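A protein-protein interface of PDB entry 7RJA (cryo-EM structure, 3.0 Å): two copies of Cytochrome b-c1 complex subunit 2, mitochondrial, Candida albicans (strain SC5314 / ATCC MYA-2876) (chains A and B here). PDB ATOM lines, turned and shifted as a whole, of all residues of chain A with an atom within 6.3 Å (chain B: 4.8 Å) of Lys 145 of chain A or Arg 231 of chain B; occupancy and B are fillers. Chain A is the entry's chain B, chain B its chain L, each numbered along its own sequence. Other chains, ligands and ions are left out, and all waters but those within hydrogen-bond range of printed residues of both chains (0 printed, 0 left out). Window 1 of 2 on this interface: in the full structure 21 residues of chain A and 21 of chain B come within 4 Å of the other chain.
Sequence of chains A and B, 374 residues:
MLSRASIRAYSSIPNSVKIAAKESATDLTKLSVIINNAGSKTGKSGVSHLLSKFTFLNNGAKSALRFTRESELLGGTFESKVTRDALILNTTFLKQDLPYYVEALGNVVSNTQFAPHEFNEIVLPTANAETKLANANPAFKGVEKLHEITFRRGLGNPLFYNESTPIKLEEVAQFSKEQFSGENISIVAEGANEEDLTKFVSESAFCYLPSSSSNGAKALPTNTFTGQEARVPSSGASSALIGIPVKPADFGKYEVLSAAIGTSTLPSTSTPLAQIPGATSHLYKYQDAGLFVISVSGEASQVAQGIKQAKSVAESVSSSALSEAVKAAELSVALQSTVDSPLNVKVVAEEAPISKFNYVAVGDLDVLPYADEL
Of chain B, only Arg 231 comes within 4 Å of Lys 145 of chain A.
Of the printed residues of chain B, Glu 148 of chain A touches Leu 365.
Of the printed residues of chain B, Arg 152 of chain A touches Glu 229 and Tyr 370.
Printed residues of chain B within 4 Å of Arg 153 of chain A: Leu 368 and Tyr 370.
Of the printed residues of chain A, Glu 229 of chain B touches Arg 152 (3.7 Å).
Arg 231 of chain B touches just one residue of chain A: Lys 145.
Of the printed residues of chain A, Tyr 370 of chain B touches Arg 152 and Arg 153.
The nearest residue of chain B that does not touch Lys 145 of chain A is Pro 233 of chain B (4.7 Å).
NZ of Lys 145 of chain A lies within salt-bridge range of OE1 of Glu 148 of chain A, 2.8 Å away.
The backbone carbonyl oxygen (O) of Leu 365 of chain B lies within hydrogen-bond range of the guanidinium group (NH1) of Arg 231 of chain B (3.0 Å).
NH2 of Arg 231 of chain B sits at hydrogen-bond distance from O of Leu 368 of chain B (2.8 Å).
The guanidinium group (NH2) of Arg 231 of chain B sits at hydrogen-bond distance from the backbone carbonyl oxygen (O) of Pro 369 of chain B.
The guanidinium group (NH1) of Arg 231 of chain B is in hydrogen-bond range of the side-chain hydroxyl (OH) of Tyr 370 of chain B (3.4 Å).
Positions printed for both chains: 230, 231 and 232.
Of the 6 pairs that touch across the chains among the printed residues, none has its exchanged pair printed and touching as well.
The side-chain amino group (NZ) of Lys 145 of chain A lies within hydrogen-bond range of the backbone carbonyl oxygen (O) of Arg 231 of chain B, 2.6 Å away.
The side-chain carboxylate (OE2) of Glu 229 of chain B lies within salt-bridge range of the guanidinium group (NH2) of Arg 152 of chain A (3.7 Å).
The side-chain hydroxyl (OH) of Tyr 370 of chain B is in hydrogen-bond range of the backbone carbonyl oxygen (O) of Arg 152 of chain A (2.8 Å).
Among the printed residues, pairs that only touch across the chains: Arg 153 of chain A with Tyr 370 of chain B (3.3 Å), Glu 148 of chain A with Leu 365 of chain B (3.5 Å) and Arg 153 of chain A with Leu 368 of chain B (3.8 Å).
Of the 18 printed residues of chain A, 4 touch a printed residue of chain B.
Printed residues of chain A that touch a printed residue of chain B: Lys 145, Glu 148, Arg 152 and Arg 153.
Among the printed residues, 6 pairs touch across the chains.
Among the printed residues, Asp or Glu carboxylates within 4 Å of a Lys or Arg side-chain nitrogen of the other chain: Arg 152 of chain A with Glu 229 of chain B (3.7 Å).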
ATOM      1  N   PHE A 140      14.054  32.058 -16.233  1.00  0.00           N
ATOM      2  CA  PHE A 140      12.599  31.996 -16.290  1.00  0.00           C
ATOM      3  C   PHE A 140      12.055  30.875 -15.415  1.00  0.00           C
ATOM      4  O   PHE A 140      11.019  31.041 -14.763  1.00  0.00           O
ATOM      5  CB  PHE A 140      12.133  31.818 -17.731  1.00  0.00           C
ATOM      6  CG  PHE A 140      10.648  31.845 -17.883  1.00  0.00           C
ATOM      7  CD1 PHE A 140       9.962  33.042 -17.836  1.00  0.00           C
ATOM      8  CD2 PHE A 140       9.937  30.679 -18.070  1.00  0.00           C
ATOM      9  CE1 PHE A 140       8.595  33.077 -17.973  1.00  0.00           C
ATOM     10  CE2 PHE A 140       8.569  30.710 -18.211  1.00  0.00           C
ATOM     11  CZ  PHE A 140       7.897  31.909 -18.160  1.00  0.00           C
ATOM     12  N   LYS A 141      12.735  29.729 -15.389  1.00  0.00           N
ATOM     13  CA  LYS A 141      12.331  28.666 -14.477  1.00  0.00           C
ATOM     14  C   LYS A 141      12.403  29.145 -13.037  1.00  0.00           C
ATOM     15  O   LYS A 141      11.497  28.886 -12.234  1.00  0.00           O
ATOM     16  CB  LYS A 141      13.226  27.446 -14.678  1.00  0.00           C
ATOM     17  CG  LYS A 141      12.730  26.195 -13.986  1.00  0.00           C
ATOM     18  CD  LYS A 141      13.724  25.052 -14.112  1.00  0.00           C
ATOM     19  CE  LYS A 141      14.022  24.716 -15.558  1.00  0.00           C
ATOM     20  NZ  LYS A 141      14.764  23.437 -15.679  1.00  0.00           N
ATOM     21  N   GLY A 142      13.476  29.857 -12.696  1.00  0.00           N
ATOM     22  CA  GLY A 142      13.596  30.392 -11.355  1.00  0.00           C
ATOM     23  C   GLY A 142      12.498  31.379 -11.027  1.00  0.00           C
ATOM     24  O   GLY A 142      11.981  31.392  -9.912  1.00  0.00           O
ATOM     25  N   VAL A 143      12.123  32.221 -11.990  1.00  0.00           N
ATOM     26  CA  VAL A 143      11.062  33.190 -11.736  1.00  0.00           C
ATOM     27  C   VAL A 143       9.728  32.483 -11.537  1.00  0.00           C
ATOM     28  O   VAL A 143       8.929  32.869 -10.674  1.00  0.00           O
ATOM     29  CB  VAL A 143      10.989  34.219 -12.873  1.00  0.00           C
ATOM     30  CG1 VAL A 143       9.703  35.007 -12.780  1.00  0.00           C
ATOM     31  CG2 VAL A 143      12.175  35.151 -12.809  1.00  0.00           C
ATOM     32  N   GLU A 144       9.451  31.452 -12.336  1.00  0.00           N
ATOM     33  CA  GLU A 144       8.217  30.697 -12.141  1.00  0.00           C
ATOM     34  C   GLU A 144       8.181  30.065 -10.758  1.00  0.00           C
ATOM     35  O   GLU A 144       7.162  30.121 -10.061  1.00  0.00           O
ATOM     36  CB  GLU A 144       8.068  29.622 -13.215  1.00  0.00           C
ATOM     37  CG  GLU A 144       7.726  30.137 -14.595  1.00  0.00           C
ATOM     38  CD  GLU A 144       6.947  29.115 -15.401  1.00  0.00           C
ATOM     39  OE1 GLU A 144       5.940  28.592 -14.881  1.00  0.00           O
ATOM     40  OE2 GLU A 144       7.348  28.814 -16.542  1.00  0.00           O
ATOM     41  N   LYS A 145       9.292  29.456 -10.341  1.00  0.00           N
ATOM     42  CA  LYS A 145       9.344  28.870  -9.006  1.00  0.00           C
ATOM     43  C   LYS A 145       9.184  29.935  -7.931  1.00  0.00           C
ATOM     44  O   LYS A 145       8.557  29.696  -6.894  1.00  0.00           O
ATOM     45  CB  LYS A 145      10.657  28.118  -8.820  1.00  0.00           C
ATOM     46  CG  LYS A 145      10.681  27.194  -7.622  1.00  0.00           C
ATOM     47  CD  LYS A 145       9.918  25.916  -7.885  1.00  0.00           C
ATOM     48  CE  LYS A 145       9.491  25.253  -6.592  1.00  0.00           C
ATOM     49  NZ  LYS A 145       8.610  24.089  -6.845  1.00  0.00           N
ATOM     50  N   LEU A 146       9.763  31.113  -8.156  1.00  0.00           N
ATOM     51  CA  LEU A 146       9.657  32.195  -7.187  1.00  0.00           C
ATOM     52  C   LEU A 146       8.214  32.638  -7.022  1.00  0.00           C
ATOM     53  O   LEU A 146       7.749  32.873  -5.902  1.00  0.00           O
ATOM     54  CB  LEU A 146      10.537  33.358  -7.639  1.00  0.00           C
ATOM     55  CG  LEU A 146      10.829  34.486  -6.662  1.00  0.00           C
ATOM     56  CD1 LEU A 146      11.309  33.944  -5.341  1.00  0.00           C
ATOM     57  CD2 LEU A 146      11.870  35.388  -7.269  1.00  0.00           C
ATOM     58  N   HIS A 147       7.487  32.758  -8.131  1.00  0.00           N
ATOM     59  CA  HIS A 147       6.066  33.071  -8.040  1.00  0.00           C
ATOM     60  C   HIS A 147       5.305  31.950  -7.351  1.00  0.00           C
ATOM     61  O   HIS A 147       4.385  32.207  -6.567  1.00  0.00           O
ATOM     62  CB  HIS A 147       5.488  33.324  -9.428  1.00  0.00           C
ATOM     63  CG  HIS A 147       5.831  34.666  -9.987  1.00  0.00           C
ATOM     64  ND1 HIS A 147       7.033  34.928 -10.606  1.00  0.00           N
ATOM     65  CD2 HIS A 147       5.132  35.822 -10.018  1.00  0.00           C
ATOM     66  CE1 HIS A 147       7.057  36.188 -10.997  1.00  0.00           C
ATOM     67  NE2 HIS A 147       5.916  36.753 -10.652  1.00  0.00           N
ATOM     68  N   GLU A 148       5.668  30.699  -7.632  1.00  0.00           N
ATOM     69  CA  GLU A 148       4.987  29.579  -6.997  1.00  0.00           C
ATOM     70  C   GLU A 148       5.135  29.630  -5.485  1.00  0.00           C
ATOM     71  O   GLU A 148       4.163  29.425  -4.751  1.00  0.00           O
ATOM     72  CB  GLU A 148       5.536  28.260  -7.532  1.00  0.00           C
ATOM     73  CG  GLU A 148       4.759  27.039  -7.081  1.00  0.00           C
ATOM     74  CD  GLU A 148       5.165  25.784  -7.824  1.00  0.00           C
ATOM     75  OE1 GLU A 148       6.361  25.430  -7.788  1.00  0.00           O
ATOM     76  OE2 GLU A 148       4.288  25.151  -8.449  1.00  0.00           O
ATOM     77  N   ILE A 149       6.348  29.902  -4.997  1.00  0.00           N
ATOM     78  CA  ILE A 149       6.596  29.872  -3.557  1.00  0.00           C
ATOM     79  C   ILE A 149       6.256  31.181  -2.863  1.00  0.00           C
ATOM     80  O   ILE A 149       6.177  31.205  -1.626  1.00  0.00           O
ATOM     81  CB  ILE A 149       8.062  29.515  -3.242  1.00  0.00           C
ATOM     82  CG1 ILE A 149       8.999  30.647  -3.651  1.00  0.00           C
ATOM     83  CG2 ILE A 149       8.451  28.236  -3.943  1.00  0.00           C
ATOM     84  CD1 ILE A 149      10.450  30.298  -3.501  1.00  0.00           C
ATOM     85  N   THR A 150       6.058  32.269  -3.606  1.00  0.00           N
ATOM     86  CA  THR A 150       5.697  33.538  -2.987  1.00  0.00           C
ATOM     87  C   THR A 150       4.190  33.747  -2.937  1.00  0.00           C
ATOM     88  O   THR A 150       3.665  34.205  -1.919  1.00  0.00           O
ATOM     89  CB  THR A 150       6.350  34.696  -3.739  1.00  0.00           C
ATOM     90  OG1 THR A 150       7.762  34.483  -3.810  1.00  0.00           O
ATOM     91  CG2 THR A 150       6.083  36.001  -3.026  1.00  0.00           C
ATOM     92  N   ARG A 152       1.254  31.347  -3.259  1.00  0.00           N
ATOM     93  CA  ARG A 152       1.120  29.900  -3.390  1.00  0.00           C
ATOM     94  C   ARG A 152       0.071  29.513  -4.427  1.00  0.00           C
ATOM     95  O   ARG A 152       0.270  28.566  -5.195  1.00  0.00           O
ATOM     96  CB  ARG A 152       0.801  29.298  -2.025  1.00  0.00           C
ATOM     97  CG  ARG A 152       1.969  29.436  -1.075  1.00  0.00           C
ATOM     98  CD  ARG A 152       1.709  28.862   0.293  1.00  0.00           C
ATOM     99  NE  ARG A 152       2.879  29.065   1.135  1.00  0.00           N
ATOM    100  CZ  ARG A 152       2.958  28.726   2.413  1.00  0.00           C
ATOM    101  NH1 ARG A 152       1.944  28.162   3.044  1.00  0.00           N
ATOM    102  NH2 ARG A 152       4.083  28.969   3.077  1.00  0.00           N
ATOM    103  N   ARG A 153      -1.040  30.238  -4.480  1.00  0.00           N
ATOM    104  CA  ARG A 153      -2.069  30.025  -5.487  1.00  0.00           C
ATOM    105  C   ARG A 153      -2.339  31.338  -6.206  1.00  0.00           C
ATOM    106  O   ARG A 153      -1.830  32.396  -5.827  1.00  0.00           O
ATOM    107  CB  ARG A 153      -3.359  29.475  -4.868  1.00  0.00           C
ATOM    108  CG  ARG A 153      -3.233  28.078  -4.297  1.00  0.00           C
ATOM    109  CD  ARG A 153      -3.071  27.045  -5.400  1.00  0.00           C
ATOM    110  NE  ARG A 153      -2.941  25.697  -4.860  1.00  0.00           N
ATOM    111  CZ  ARG A 153      -3.961  24.890  -4.612  1.00  0.00           C
ATOM    112  NH1 ARG A 153      -5.210  25.254  -4.855  1.00  0.00           N
ATOM    113  NH2 ARG A 153      -3.725  23.686  -4.098  1.00  0.00           N
ATOM    114  N   ALA A 230      13.264  27.717  -2.348  1.00  0.00           N
ATOM    115  CA  ALA A 230      13.115  26.537  -3.182  1.00  0.00           C
ATOM    116  C   ALA A 230      14.412  26.301  -3.935  1.00  0.00           C
ATOM    117  O   ALA A 230      15.281  27.170  -4.001  1.00  0.00           O
ATOM    118  CB  ALA A 230      11.949  26.684  -4.162  1.00  0.00           C
ATOM    119  N   ARG A 231      14.540  25.101  -4.490  1.00  0.00           N
ATOM    120  CA  ARG A 231      15.693  24.745  -5.304  1.00  0.00           C
ATOM    121  C   ARG A 231      15.229  23.831  -6.421  1.00  0.00           C
ATOM    122  O   ARG A 231      14.513  22.858  -6.170  1.00  0.00           O
ATOM    123  CB  ARG A 231      16.778  24.056  -4.472  1.00  0.00           C
ATOM    124  CG  ARG A 231      17.021  24.702  -3.125  1.00  0.00           C
ATOM    125  CD  ARG A 231      17.990  23.892  -2.293  1.00  0.00           C
ATOM    126  NE  ARG A 231      19.334  23.896  -2.852  1.00  0.00           N
ATOM    127  CZ  ARG A 231      20.110  24.968  -2.933  1.00  0.00           C
ATOM    128  NH1 ARG A 231      19.716  26.143  -2.474  1.00  0.00           N
ATOM    129  NH2 ARG A 231      21.316  24.855  -3.478  1.00  0.00           N
ATOM    130  N   VAL A 232      15.636  24.144  -7.646  1.00  0.00           N
ATOM    131  CA  VAL A 232      15.180  23.418  -8.825  1.00  0.00           C
ATOM    132  C   VAL A 232      16.397  22.962  -9.619  1.00  0.00           C
ATOM    133  O   VAL A 232      16.919  23.737 -10.429  1.00  0.00           O
ATOM    134  CB  VAL A 232      14.265  24.291  -9.697  1.00  0.00           C
ATOM    135  CG1 VAL A 232      13.714  23.483 -10.850  1.00  0.00           C
ATOM    136  CG2 VAL A 232      13.141  24.885  -8.871  1.00  0.00           C
ATOM    137  N   VAL A 360      15.346  31.356  -4.530  1.00  0.00           N
ATOM    138  CA  VAL A 360      15.238  30.160  -5.358  1.00  0.00           C
ATOM    139  C   VAL A 360      16.542  29.960  -6.115  1.00  0.00           C
ATOM    140  O   VAL A 360      17.107  30.915  -6.654  1.00  0.00           O
ATOM    141  CB  VAL A 360      14.050  30.235  -6.332  1.00  0.00           C
ATOM    142  CG1 VAL A 360      14.230  31.367  -7.291  1.00  0.00           C
ATOM    143  CG2 VAL A 360      13.916  28.938  -7.088  1.00  0.00           C
ATOM    144  N   VAL A 362      18.654  27.459  -9.040  1.00  0.00           N
ATOM    145  CA  VAL A 362      18.485  26.566 -10.176  1.00  0.00           C
ATOM    146  C   VAL A 362      19.862  26.248 -10.731  1.00  0.00           C
ATOM    147  O   VAL A 362      20.713  27.135 -10.835  1.00  0.00           O
ATOM    148  CB  VAL A 362      17.597  27.197 -11.265  1.00  0.00           C
ATOM    149  CG1 VAL A 362      17.322  26.202 -12.369  1.00  0.00           C
ATOM    150  CG2 VAL A 362      16.305  27.708 -10.664  1.00  0.00           C
ATOM    151  N   GLU B 229       9.456  23.145   3.260  1.00  0.00           N
ATOM    152  CA  GLU B 229       8.611  22.404   2.337  1.00  0.00           C
ATOM    153  C   GLU B 229       9.117  22.628   0.922  1.00  0.00           C
ATOM    154  O   GLU B 229       9.870  23.565   0.651  1.00  0.00           O
ATOM    155  CB  GLU B 229       7.143  22.817   2.440  1.00  0.00           C
ATOM    156  CG  GLU B 229       6.902  24.300   2.273  1.00  0.00           C
ATOM    157  CD  GLU B 229       5.487  24.700   2.631  1.00  0.00           C
ATOM    158  OE1 GLU B 229       4.544  24.159   2.017  1.00  0.00           O
ATOM    159  OE2 GLU B 229       5.318  25.554   3.526  1.00  0.00           O
ATOM    160  N   ALA B 230       8.688  21.751   0.018  1.00  0.00           N
ATOM    161  CA  ALA B 230       9.102  21.824  -1.372  1.00  0.00           C
ATOM    162  C   ALA B 230       8.034  21.172  -2.233  1.00  0.00           C
ATOM    163  O   ALA B 230       7.190  20.421  -1.743  1.00  0.00           O
ATOM    164  CB  ALA B 230      10.455  21.146  -1.595  1.00  0.00           C
ATOM    165  N   ARG B 231       8.074  21.476  -3.524  1.00  0.00           N
ATOM    166  CA  ARG B 231       7.116  20.919  -4.466  1.00  0.00           C
ATOM    167  C   ARG B 231       7.843  20.634  -5.767  1.00  0.00           C
ATOM    168  O   ARG B 231       8.542  21.505  -6.289  1.00  0.00           O
ATOM    169  CB  ARG B 231       5.951  21.881  -4.699  1.00  0.00           C
ATOM    170  CG  ARG B 231       5.505  22.589  -3.438  1.00  0.00           C
ATOM    171  CD  ARG B 231       4.149  23.236  -3.592  1.00  0.00           C
ATOM    172  NE  ARG B 231       3.085  22.345  -3.148  1.00  0.00           N
ATOM    173  CZ  ARG B 231       1.972  22.089  -3.823  1.00  0.00           C
ATOM    174  NH1 ARG B 231       1.720  22.654  -4.992  1.00  0.00           N
ATOM    175  NH2 ARG B 231       1.084  21.245  -3.307  1.00  0.00           N
ATOM    176  N   VAL B 232       7.681  19.422  -6.283  1.00  0.00           N
ATOM    177  CA  VAL B 232       8.406  18.982  -7.469  1.00  0.00           C
ATOM    178  C   VAL B 232       7.404  18.491  -8.505  1.00  0.00           C
ATOM    179  O   VAL B 232       6.965  17.336  -8.426  1.00  0.00           O
ATOM    180  CB  VAL B 232       9.417  17.881  -7.119  1.00  0.00           C
ATOM    181  CG1 VAL B 232      10.091  17.361  -8.375  1.00  0.00           C
ATOM    182  CG2 VAL B 232      10.441  18.400  -6.135  1.00  0.00           C
ATOM    183  N   PRO B 233       7.020  19.298  -9.490  1.00  0.00           N
ATOM    184  CA  PRO B 233       6.017  18.835 -10.452  1.00  0.00           C
ATOM    185  C   PRO B 233       6.491  17.591 -11.185  1.00  0.00           C
ATOM    186  O   PRO B 233       7.674  17.435 -11.491  1.00  0.00           O
ATOM    187  CB  PRO B 233       5.857  20.026 -11.401  1.00  0.00           C
ATOM    188  CG  PRO B 233       7.130  20.764 -11.293  1.00  0.00           C
ATOM    189  CD  PRO B 233       7.578  20.605  -9.875  1.00  0.00           C
ATOM    190  N   TYR B 359       7.543  18.955   4.517  1.00  0.00           N
ATOM    191  CA  TYR B 359       6.535  18.439   3.602  1.00  0.00           C
ATOM    192  C   TYR B 359       7.035  18.552   2.173  1.00  0.00           C
ATOM    193  O   TYR B 359       7.736  19.506   1.830  1.00  0.00           O
ATOM    194  CB  TYR B 359       5.216  19.197   3.764  1.00  0.00           C
ATOM    195  CG  TYR B 359       4.169  18.850   2.739  1.00  0.00           C
ATOM    196  CD1 TYR B 359       3.435  17.682   2.841  1.00  0.00           C
ATOM    197  CD2 TYR B 359       3.904  19.696   1.679  1.00  0.00           C
ATOM    198  CE1 TYR B 359       2.475  17.363   1.914  1.00  0.00           C
ATOM    199  CE2 TYR B 359       2.945  19.383   0.744  1.00  0.00           C
ATOM    200  CZ  TYR B 359       2.234  18.216   0.868  1.00  0.00           C
ATOM    201  OH  TYR B 359       1.274  17.898  -0.060  1.00  0.00           O
ATOM    202  N   ALA B 361       5.644  17.762  -2.009  1.00  0.00           N
ATOM    203  CA  ALA B 361       4.593  17.384  -2.942  1.00  0.00           C
ATOM    204  C   ALA B 361       5.197  17.145  -4.317  1.00  0.00           C
ATOM    205  O   ALA B 361       6.079  17.888  -4.754  1.00  0.00           O
ATOM    206  CB  ALA B 361       3.517  18.464  -3.026  1.00  0.00           C
ATOM    207  N   LEU B 365       0.699  19.482  -8.828  1.00  0.00           N
ATOM    208  CA  LEU B 365       0.804  20.472  -7.764  1.00  0.00           C
ATOM    209  C   LEU B 365      -0.439  21.338  -7.648  1.00  0.00           C
ATOM    210  O   LEU B 365      -0.653  21.955  -6.600  1.00  0.00           O
ATOM    211  CB  LEU B 365       2.023  21.360  -7.992  1.00  0.00           C
ATOM    212  CG  LEU B 365       3.327  20.866  -7.375  1.00  0.00           C
ATOM    213  CD1 LEU B 365       3.538  19.401  -7.663  1.00  0.00           C
ATOM    214  CD2 LEU B 365       4.488  21.682  -7.906  1.00  0.00           C
ATOM    215  N   LEU B 368      -2.361  18.794  -5.138  1.00  0.00           N
ATOM    216  CA  LEU B 368      -1.776  18.364  -3.876  1.00  0.00           C
ATOM    217  C   LEU B 368      -1.826  19.497  -2.854  1.00  0.00           C
ATOM    218  O   LEU B 368      -1.669  20.668  -3.216  1.00  0.00           O
ATOM    219  CB  LEU B 368      -0.334  17.906  -4.084  1.00  0.00           C
ATOM    220  CG  LEU B 368      -0.191  16.422  -4.403  1.00  0.00           C
ATOM    221  CD1 LEU B 368      -0.831  16.100  -5.733  1.00  0.00           C
ATOM    222  CD2 LEU B 368       1.266  16.029  -4.409  1.00  0.00           C
ATOM    223  N   PRO B 369      -2.039  19.191  -1.579  1.00  0.00           N
ATOM    224  CA  PRO B 369      -2.152  20.243  -0.569  1.00  0.00           C
ATOM    225  C   PRO B 369      -0.800  20.841  -0.214  1.00  0.00           C
ATOM    226  O   PRO B 369       0.257  20.269  -0.480  1.00  0.00           O
ATOM    227  CB  PRO B 369      -2.754  19.510   0.633  1.00  0.00           C
ATOM    228  CG  PRO B 369      -2.296  18.114   0.473  1.00  0.00           C
ATOM    229  CD  PRO B 369      -2.275  17.858  -1.002  1.00  0.00           C
ATOM    230  N   TYR B 370      -0.853  22.016   0.402  1.00  0.00           N
ATOM    231  CA  TYR B 370       0.336  22.693   0.894  1.00  0.00           C
ATOM    232  C   TYR B 370       0.588  22.315   2.348  1.00  0.00           C
ATOM    233  O   TYR B 370      -0.248  21.699   3.011  1.00  0.00           O
ATOM    234  CB  TYR B 370       0.197  24.209   0.750  1.00  0.00           C
ATOM    235  CG  TYR B 370       0.417  24.696  -0.659  1.00  0.00           C
ATOM    236  CD1 TYR B 370      -0.605  24.650  -1.591  1.00  0.00           C
ATOM    237  CD2 TYR B 370       1.651  25.176  -1.065  1.00  0.00           C
ATOM    238  CE1 TYR B 370      -0.409  25.084  -2.879  1.00  0.00           C
ATOM    239  CE2 TYR B 370       1.856  25.611  -2.355  1.00  0.00           C
ATOM    240  CZ  TYR B 370       0.822  25.563  -3.257  1.00  0.00           C
ATOM    241  OH  TYR B 370       1.016  25.992  -4.549  1.00  0.00           O
